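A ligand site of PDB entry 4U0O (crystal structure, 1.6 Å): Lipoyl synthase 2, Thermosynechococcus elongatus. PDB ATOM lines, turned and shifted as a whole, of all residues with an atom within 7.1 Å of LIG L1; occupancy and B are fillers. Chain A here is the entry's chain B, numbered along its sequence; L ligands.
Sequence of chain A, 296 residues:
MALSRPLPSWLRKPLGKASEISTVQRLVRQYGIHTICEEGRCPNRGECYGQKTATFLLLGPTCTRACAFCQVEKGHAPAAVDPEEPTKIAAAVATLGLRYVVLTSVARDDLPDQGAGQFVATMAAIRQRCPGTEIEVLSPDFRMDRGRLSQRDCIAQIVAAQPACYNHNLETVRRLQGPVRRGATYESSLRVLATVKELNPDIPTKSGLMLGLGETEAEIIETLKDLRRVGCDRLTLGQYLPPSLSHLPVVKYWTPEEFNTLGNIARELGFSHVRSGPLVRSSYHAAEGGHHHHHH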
ATOM      1  N   ILE A  36      32.512 -19.580  24.256  1.00  0.00           N
ATOM      2  CA  ILE A  36      31.731 -18.725  23.371  1.00  0.00           C
ATOM      3  C   ILE A  36      32.460 -18.898  22.046  1.00  0.00           C
ATOM      4  O   ILE A  36      31.862 -18.740  20.971  1.00  0.00           O
ATOM      5  CB  ILE A  36      31.630 -17.250  23.854  1.00  0.00           C
ATOM      6  CG1 ILE A  36      30.647 -16.466  22.987  1.00  0.00           C
ATOM      7  CG2 ILE A  36      32.990 -16.599  23.769  1.00  0.00           C
ATOM      8  CD1 ILE A  36      29.243 -17.033  22.953  1.00  0.00           C
ATOM      9  N   LEU A  57      32.275 -19.756  28.304  1.00  0.00           N
ATOM     10  CA  LEU A  57      30.932 -19.206  28.446  1.00  0.00           C
ATOM     11  C   LEU A  57      30.276 -19.831  29.653  1.00  0.00           C
ATOM     12  O   LEU A  57      30.023 -21.050  29.670  1.00  0.00           O
ATOM     13  CB  LEU A  57      30.073 -19.521  27.229  1.00  0.00           C
ATOM     14  CG  LEU A  57      28.615 -19.019  27.289  1.00  0.00           C
ATOM     15  CD1 LEU A  57      28.565 -17.529  27.106  1.00  0.00           C
ATOM     16  CD2 LEU A  57      27.777 -19.736  26.213  1.00  0.00           C
ATOM     17  N   THR A  62      22.410 -21.716  26.716  1.00  0.00           N
ATOM     18  CA  THR A  62      21.386 -20.905  26.105  1.00  0.00           C
ATOM     19  C   THR A  62      21.262 -19.584  26.840  1.00  0.00           C
ATOM     20  O   THR A  62      21.586 -19.525  28.011  1.00  0.00           O
ATOM     21  CB  THR A  62      19.998 -21.594  26.131  1.00  0.00           C
ATOM     22  OG1 THR A  62      19.004 -20.642  25.748  1.00  0.00           O
ATOM     23  CG2 THR A  62      19.672 -22.083  27.504  1.00  0.00           C
ATOM     24  N   CYS A  63      20.819 -18.543  26.140  1.00  0.00           N
ATOM     25  CA  CYS A  63      20.549 -17.240  26.747  1.00  0.00           C
ATOM     26  C   CYS A  63      19.094 -16.862  26.495  1.00  0.00           C
ATOM     27  O   CYS A  63      18.539 -17.219  25.447  1.00  0.00           O
ATOM     28  CB  CYS A  63      21.417 -16.125  26.110  1.00  0.00           C
ATOM     29  SG  CYS A  63      21.341 -14.426  26.910  1.00  0.00           S
ATOM     30  N   THR A  64      18.505 -16.111  27.398  1.00  0.00           N
ATOM     31  CA  THR A  64      17.109 -15.736  27.270  1.00  0.00           C
ATOM     32  C   THR A  64      16.953 -14.376  26.598  1.00  0.00           C
ATOM     33  O   THR A  64      15.861 -14.076  26.092  1.00  0.00           O
ATOM     34  CB  THR A  64      16.364 -15.726  28.641  1.00  0.00           C
ATOM     35  OG1 THR A  64      17.000 -14.803  29.547  1.00  0.00           O
ATOM     36  CG2 THR A  64      16.324 -17.115  29.238  1.00  0.00           C
ATOM     37  N   ARG A  65      18.019 -13.566  26.570  1.00  0.00           N
ATOM     38  CA  ARG A  65      17.916 -12.247  25.940  1.00  0.00           C
ATOM     39  C   ARG A  65      17.857 -12.394  24.453  1.00  0.00           C
ATOM     40  O   ARG A  65      17.946 -13.481  23.933  1.00  0.00           O
ATOM     41  CB  ARG A  65      19.047 -11.309  26.339  1.00  0.00           C
ATOM     42  CG  ARG A  65      18.944 -10.805  27.769  1.00  0.00           C
ATOM     43  CD  ARG A  65      19.725  -9.515  27.967  1.00  0.00           C
ATOM     44  NE  ARG A  65      19.734  -9.086  29.350  1.00  0.00           N
ATOM     45  CZ  ARG A  65      20.477  -8.085  29.831  1.00  0.00           C
ATOM     46  NH1 ARG A  65      21.269  -7.393  29.017  1.00  0.00           N
ATOM     47  NH2 ARG A  65      20.418  -7.793  31.111  1.00  0.00           N
ATOM     48  N   ALA A  66      17.714 -11.263  23.776  1.00  0.00           N
ATOM     49  CA  ALA A  66      17.304 -11.276  22.371  1.00  0.00           C
ATOM     50  C   ALA A  66      18.286 -10.607  21.414  1.00  0.00           C
ATOM     51  O   ALA A  66      17.899 -10.292  20.302  1.00  0.00           O
ATOM     52  CB  ALA A  66      15.937 -10.589  22.246  1.00  0.00           C
ATOM     53  N   CYS A  67      19.556 -10.403  21.812  1.00  0.00           N
ATOM     54  CA  CYS A  67      20.474  -9.625  20.979  1.00  0.00           C
ATOM     55  C   CYS A  67      20.533 -10.162  19.561  1.00  0.00           C
ATOM     56  O   CYS A  67      20.811 -11.325  19.339  1.00  0.00           O
ATOM     57  CB  CYS A  67      21.865  -9.536  21.553  1.00  0.00           C
ATOM     58  SG  CYS A  67      21.860  -9.009  23.256  1.00  0.00           S
ATOM     59  N   ALA A  68      20.229  -9.311  18.590  1.00  0.00           N
ATOM     60  CA  ALA A  68      20.048  -9.825  17.245  1.00  0.00           C
ATOM     61  C   ALA A  68      21.347 -10.247  16.533  1.00  0.00           C
ATOM     62  O   ALA A  68      21.311 -10.985  15.542  1.00  0.00           O
ATOM     63  CB  ALA A  68      19.269  -8.801  16.402  1.00  0.00           C
ATOM     64  N   PHE A  69      22.490  -9.786  17.040  1.00  0.00           N
ATOM     65  CA  PHE A  69      23.775 -10.106  16.441  1.00  0.00           C
ATOM     66  C   PHE A  69      24.389 -11.404  16.954  1.00  0.00           C
ATOM     67  O   PHE A  69      25.330 -11.936  16.371  1.00  0.00           O
ATOM     68  CB  PHE A  69      24.764  -8.963  16.720  1.00  0.00           C
ATOM     69  CG  PHE A  69      25.144  -8.823  18.164  1.00  0.00           C
ATOM     70  CD1 PHE A  69      26.164  -9.591  18.702  1.00  0.00           C
ATOM     71  CD2 PHE A  69      24.480  -7.914  18.992  1.00  0.00           C
ATOM     72  CE1 PHE A  69      26.509  -9.458  20.048  1.00  0.00           C
ATOM     73  CE2 PHE A  69      24.827  -7.778  20.294  1.00  0.00           C
ATOM     74  CZ  PHE A  69      25.848  -8.563  20.829  1.00  0.00           C
ATOM     75  N   CYS A  70      23.839 -11.922  18.052  1.00  0.00           N
ATOM     76  CA  CYS A  70      24.521 -12.963  18.810  1.00  0.00           C
ATOM     77  C   CYS A  70      24.095 -14.392  18.462  1.00  0.00           C
ATOM     78  O   CYS A  70      22.900 -14.697  18.366  1.00  0.00           O
ATOM     79  CB  CYS A  70      24.280 -12.695  20.271  1.00  0.00           C
ATOM     80  SG  CYS A  70      25.082 -13.866  21.402  1.00  0.00           S
ATOM     81  N   GLN A  71      25.077 -15.263  18.318  1.00  0.00           N
ATOM     82  CA  GLN A  71      24.844 -16.625  17.844  1.00  0.00           C
ATOM     83  C   GLN A  71      24.623 -17.622  18.971  1.00  0.00           C
ATOM     84  O   GLN A  71      24.439 -18.802  18.731  1.00  0.00           O
ATOM     85  CB  GLN A  71      25.985 -17.090  16.953  1.00  0.00           C
ATOM     86  CG  GLN A  71      26.018 -16.414  15.576  1.00  0.00           C
ATOM     87  CD  GLN A  71      26.914 -17.138  14.567  1.00  0.00           C
ATOM     88  OE1 GLN A  71      26.629 -17.159  13.361  1.00  0.00           O
ATOM     89  NE2 GLN A  71      28.020 -17.727  15.049  1.00  0.00           N
ATOM     90  N   VAL A  72      24.610 -17.162  20.215  1.00  0.00           N
ATOM     91  CA  VAL A  72      24.298 -18.093  21.281  1.00  0.00           C
ATOM     92  C   VAL A  72      22.858 -18.569  21.070  1.00  0.00           C
ATOM     93  O   VAL A  72      21.973 -17.767  20.757  1.00  0.00           O
ATOM     94  CB  VAL A  72      24.520 -17.452  22.653  1.00  0.00           C
ATOM     95  CG1 VAL A  72      23.970 -18.331  23.732  1.00  0.00           C
ATOM     96  CG2 VAL A  72      26.015 -17.217  22.844  1.00  0.00           C
ATOM     97  N   LYS A  74      19.206 -19.408  21.656  1.00  0.00           N
ATOM     98  CA  LYS A  74      18.227 -18.778  22.523  1.00  0.00           C
ATOM     99  C   LYS A  74      17.325 -19.821  23.144  1.00  0.00           C
ATOM    100  O   LYS A  74      17.175 -20.917  22.588  1.00  0.00           O
ATOM    101  CB  LYS A  74      17.375 -17.800  21.720  1.00  0.00           C
ATOM    102  CG  LYS A  74      18.173 -16.727  20.976  1.00  0.00           C
ATOM    103  CD  LYS A  74      18.853 -15.773  21.943  1.00  0.00           C
ATOM    104  CE  LYS A  74      19.518 -14.612  21.207  1.00  0.00           C
ATOM    105  NZ  LYS A  74      20.877 -14.995  20.739  1.00  0.00           N
ATOM    106  N   THR A 104      33.330 -15.281  30.147  1.00  0.00           N
ATOM    107  CA  THR A 104      32.127 -14.513  29.847  1.00  0.00           C
ATOM    108  C   THR A 104      30.898 -15.319  30.258  1.00  0.00           C
ATOM    109  O   THR A 104      31.013 -16.433  30.769  1.00  0.00           O
ATOM    110  CB  THR A 104      32.087 -14.056  28.372  1.00  0.00           C
ATOM    111  OG1 THR A 104      31.089 -13.032  28.232  1.00  0.00           O
ATOM    112  CG2 THR A 104      31.790 -15.201  27.415  1.00  0.00           C
ATOM    113  N   SER A 105      29.711 -14.761  30.047  1.00  0.00           N
ATOM    114  CA  SER A 105      28.503 -15.489  30.353  1.00  0.00           C
ATOM    115  C   SER A 105      27.371 -14.983  29.492  1.00  0.00           C
ATOM    116  O   SER A 105      27.455 -13.947  28.851  1.00  0.00           O
ATOM    117  CB  SER A 105      28.103 -15.311  31.825  1.00  0.00           C
ATOM    118  OG  SER A 105      27.651 -14.014  32.107  1.00  0.00           O
ATOM    119  N   VAL A 106      26.309 -15.771  29.467  1.00  0.00           N
ATOM    120  CA  VAL A 106      25.038 -15.286  28.939  1.00  0.00           C
ATOM    121  C   VAL A 106      24.453 -14.350  30.020  1.00  0.00           C
ATOM    122  O   VAL A 106      24.887 -14.385  31.184  1.00  0.00           O
ATOM    123  CB  VAL A 106      24.088 -16.445  28.659  1.00  0.00           C
ATOM    124  CG1 VAL A 106      24.695 -17.410  27.644  1.00  0.00           C
ATOM    125  CG2 VAL A 106      23.707 -17.150  29.946  1.00  0.00           C
ATOM    126  N   ALA A 107      23.462 -13.520  29.657  1.00  0.00           N
ATOM    127  CA  ALA A 107      22.774 -12.694  30.677  1.00  0.00           C
ATOM    128  C   ALA A 107      21.883 -13.609  31.460  1.00  0.00           C
ATOM    129  O   ALA A 107      21.235 -14.467  30.868  1.00  0.00           O
ATOM    130  CB  ALA A 107      21.909 -11.580  30.053  1.00  0.00           C
ATOM    131  N   ARG A 108      21.865 -13.463  32.780  1.00  0.00           N
ATOM    132  CA  ARG A 108      21.030 -14.259  33.666  1.00  0.00           C
ATOM    133  C   ARG A 108      20.124 -13.354  34.524  1.00  0.00           C
ATOM    134  O   ARG A 108      20.292 -13.218  35.747  1.00  0.00           O
ATOM    135  CB  ARG A 108      21.878 -15.179  34.533  1.00  0.00           C
ATOM    136  CG  ARG A 108      22.607 -16.252  33.747  1.00  0.00           C
ATOM    137  CD  ARG A 108      21.662 -17.223  33.061  1.00  0.00           C
ATOM    138  NE  ARG A 108      20.794 -17.895  34.031  1.00  0.00           N
ATOM    139  CZ  ARG A 108      20.881 -19.168  34.414  1.00  0.00           C
ATOM    140  NH1 ARG A 108      21.783 -20.003  33.903  1.00  0.00           N
ATOM    141  NH2 ARG A 108      20.003 -19.618  35.322  1.00  0.00           N
ATOM    142  N   PRO A 140      28.240  -9.405  31.397  1.00  0.00           N
ATOM    143  CA  PRO A 140      27.021  -8.700  31.022  1.00  0.00           C
ATOM    144  C   PRO A 140      26.872  -7.425  31.809  1.00  0.00           C
ATOM    145  O   PRO A 140      27.713  -7.026  32.608  1.00  0.00           O
ATOM    146  CB  PRO A 140      25.882  -9.659  31.388  1.00  0.00           C
ATOM    147  CG  PRO A 140      26.526 -10.831  32.022  1.00  0.00           C
ATOM    148  CD  PRO A 140      27.958 -10.521  32.301  1.00  0.00           C
ATOM    149  N   GLU A 171      29.191  -2.454  21.982  1.00  0.00           N
ATOM    150  CA  GLU A 171      28.700  -3.113  20.771  1.00  0.00           C
ATOM    151  C   GLU A 171      28.392  -2.173  19.609  1.00  0.00           C
ATOM    152  O   GLU A 171      28.872  -2.430  18.518  1.00  0.00           O
ATOM    153  CB  GLU A 171      27.482  -3.968  20.975  1.00  0.00           C
ATOM    154  CG  GLU A 171      27.656  -4.972  22.137  1.00  0.00           C
ATOM    155  CD  GLU A 171      28.635  -6.081  21.879  1.00  0.00           C
ATOM    156  OE1 GLU A 171      28.653  -7.070  22.709  1.00  0.00           O
ATOM    157  OE2 GLU A 171      29.444  -5.999  20.941  1.00  0.00           O
ATOM    158  N   VAL A 180      20.065  -3.391  17.738  1.00  0.00           N
ATOM    159  CA  VAL A 180      21.222  -4.233  17.827  1.00  0.00           C
ATOM    160  C   VAL A 180      21.220  -5.061  19.106  1.00  0.00           C
ATOM    161  O   VAL A 180      21.627  -6.220  19.049  1.00  0.00           O
ATOM    162  CB  VAL A 180      22.538  -3.403  17.752  1.00  0.00           C
ATOM    163  CG1 VAL A 180      23.743  -4.242  18.082  1.00  0.00           C
ATOM    164  CG2 VAL A 180      22.682  -2.793  16.352  1.00  0.00           C
ATOM    165  N   ARG A 181      20.794  -4.474  20.238  1.00  0.00           N
ATOM    166  CA  ARG A 181      20.898  -5.101  21.569  1.00  0.00           C
ATOM    167  C   ARG A 181      19.629  -4.879  22.345  1.00  0.00           C
ATOM    168  O   ARG A 181      19.684  -4.339  23.464  1.00  0.00           O
ATOM    169  CB  ARG A 181      21.943  -4.385  22.413  1.00  0.00           C
ATOM    170  CG  ARG A 181      23.161  -3.971  21.803  1.00  0.00           C
ATOM    171  CD  ARG A 181      23.896  -3.073  22.735  1.00  0.00           C
ATOM    172  NE  ARG A 181      24.520  -3.854  23.819  1.00  0.00           N
ATOM    173  CZ  ARG A 181      24.980  -3.341  24.949  1.00  0.00           C
ATOM    174  NH1 ARG A 181      24.848  -2.070  25.228  1.00  0.00           N
ATOM    175  NH2 ARG A 181      25.548  -4.161  25.849  1.00  0.00           N
ATOM    176  N   ARG A 182      18.471  -5.190  21.760  1.00  0.00           N
ATOM    177  CA  ARG A 182      17.205  -4.990  22.436  1.00  0.00           C
ATOM    178  C   ARG A 182      17.248  -5.566  23.829  1.00  0.00           C
ATOM    179  O   ARG A 182      17.193  -6.782  23.997  1.00  0.00           O
ATOM    180  CB  ARG A 182      16.107  -5.667  21.654  1.00  0.00           C
ATOM    181  CG  ARG A 182      14.762  -4.967  21.684  1.00  0.00           C
ATOM    182  CD  ARG A 182      13.974  -5.343  20.435  1.00  0.00           C
ATOM    183  NE  ARG A 182      14.194  -6.749  20.084  1.00  0.00           N
ATOM    184  CZ  ARG A 182      15.122  -7.206  19.224  1.00  0.00           C
ATOM    185  NH1 ARG A 182      15.927  -6.358  18.585  1.00  0.00           N
ATOM    186  NH2 ARG A 182      15.236  -8.500  19.003  1.00  0.00           N
HETATM  187 FE1  LIG L   1      25.280 -11.440  25.663  1.00  0.00          FE
HETATM  188 FE2  LIG L   1      24.371 -12.980  23.443  1.00  0.00          FE
HETATM  189 FE3  LIG L   1      23.029 -10.749  24.184  1.00  0.00          FE
HETATM  190 FE4  LIG L   1      22.798 -13.159  25.570  1.00  0.00          FE
HETATM  191  S1  LIG L   1      22.208 -12.633  23.570  1.00  0.00           S
HETATM  192  S2  LIG L   1      23.184 -11.185  26.298  1.00  0.00           S
HETATM  193  S3  LIG L   1      24.953 -13.643  25.422  1.00  0.00           S
HETATM  194  S4  LIG L   1      25.122 -10.926  23.542  1.00  0.00           S
HETATM  195  C1  LG2 L   2      34.548 -11.851  22.135  1.00  0.00           C
HETATM  196  S1  LG2 L   2      33.129 -12.835  22.162  1.00  0.00           S
HETATM  197  C2  LG2 L   2      31.749 -11.715  22.393  1.00  0.00           C
HETATM  198  C3  LG2 L   2      31.834 -10.499  21.506  1.00  0.00           C
HETATM  199  O1  LG2 L   2      32.158 -10.856  20.099  1.00  0.00           O
HETATM  200  C4  LG2 L   2      30.576  -9.021  20.230  1.00  0.00           C
HETATM  201  O2  LG2 L   2      31.189  -7.751  20.532  1.00  0.00           O
HETATM  202  C5  LG2 L   2      30.526  -9.832  21.502  1.00  0.00           C
HETATM  203  O3  LG2 L   2      30.332  -9.065  22.732  1.00  0.00           O
HETATM  204  C6  LG2 L   2      31.395  -9.874  19.295  1.00  0.00           C
HETATM  205  N1  LG2 L   2      30.517 -10.528  18.437  1.00  0.00           N
HETATM  206  C7  LG2 L   2      29.471 -11.292  18.730  1.00  0.00           C
HETATM  207  N2  LG2 L   2      28.790 -11.655  17.650  1.00  0.00           N
HETATM  208  C8  LG2 L   2      29.365 -11.049  16.620  1.00  0.00           C
HETATM  209  C9  LG2 L   2      29.114 -11.014  15.219  1.00  0.00           C
HETATM  210  N3  LG2 L   2      27.984 -11.747  14.691  1.00  0.00           N
HETATM  211  N4  LG2 L   2      29.959 -10.302  14.467  1.00  0.00           N
HETATM  212  C10 LG2 L   2      31.010  -9.592  14.971  1.00  0.00           C
HETATM  213  N5  LG2 L   2      31.294  -9.609  16.287  1.00  0.00           N
HETATM  214  C11 LG2 L   2      30.486 -10.296  17.098  1.00  0.00           C
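The side-chain sulfur (SG) of Cys 70 is bound to an iron atom (FE2) of LIG L1. The side-chain carboxylate of Glu 171 sits at hydrogen-bond distance from an oxygen (O2) of LG2 L2, at 2.5 Å. A nitrogen (N3) of LG2 L2 is in hydrogen-bond range of the backbone carbonyl oxygen (O) of Phe 69 (3.1 Å). An iron atom (FE3) of LIG L1 is bound by the side-chain sulfur (SG) of Cys 67 (2.3 Å). FE4 of LIG L1 is bound by SG of Cys 63.
Merely in contact with LIG L1: Phe 69, Val 106, Lys 74 and Ala 107. Hydrophobic or aromatic side chains within 4 Å of LIG L1: Phe 69 and Ala 107.
The backbone NH of Ala 107 lies close to the side-chain sulfur of Cys 63 (3.6 Å). The backbone NH (N) of Val 72 lies close to the side-chain sulfur (SG) of Cys 70. The side-chain amino group (NZ) of Lys 74 is in hydrogen-bond range of the backbone carbonyl oxygen (O) of Cys 70, 3.1 Å away. The side-chain amino group (NZ) of Lys 74 lies within hydrogen-bond range of the backbone carbonyl oxygen (O) of Val 72, 3.0 Å away. The backbone NH (N) of Arg 65 lies close to the side-chain sulfur (SG) of Cys 63 (3.4 Å).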
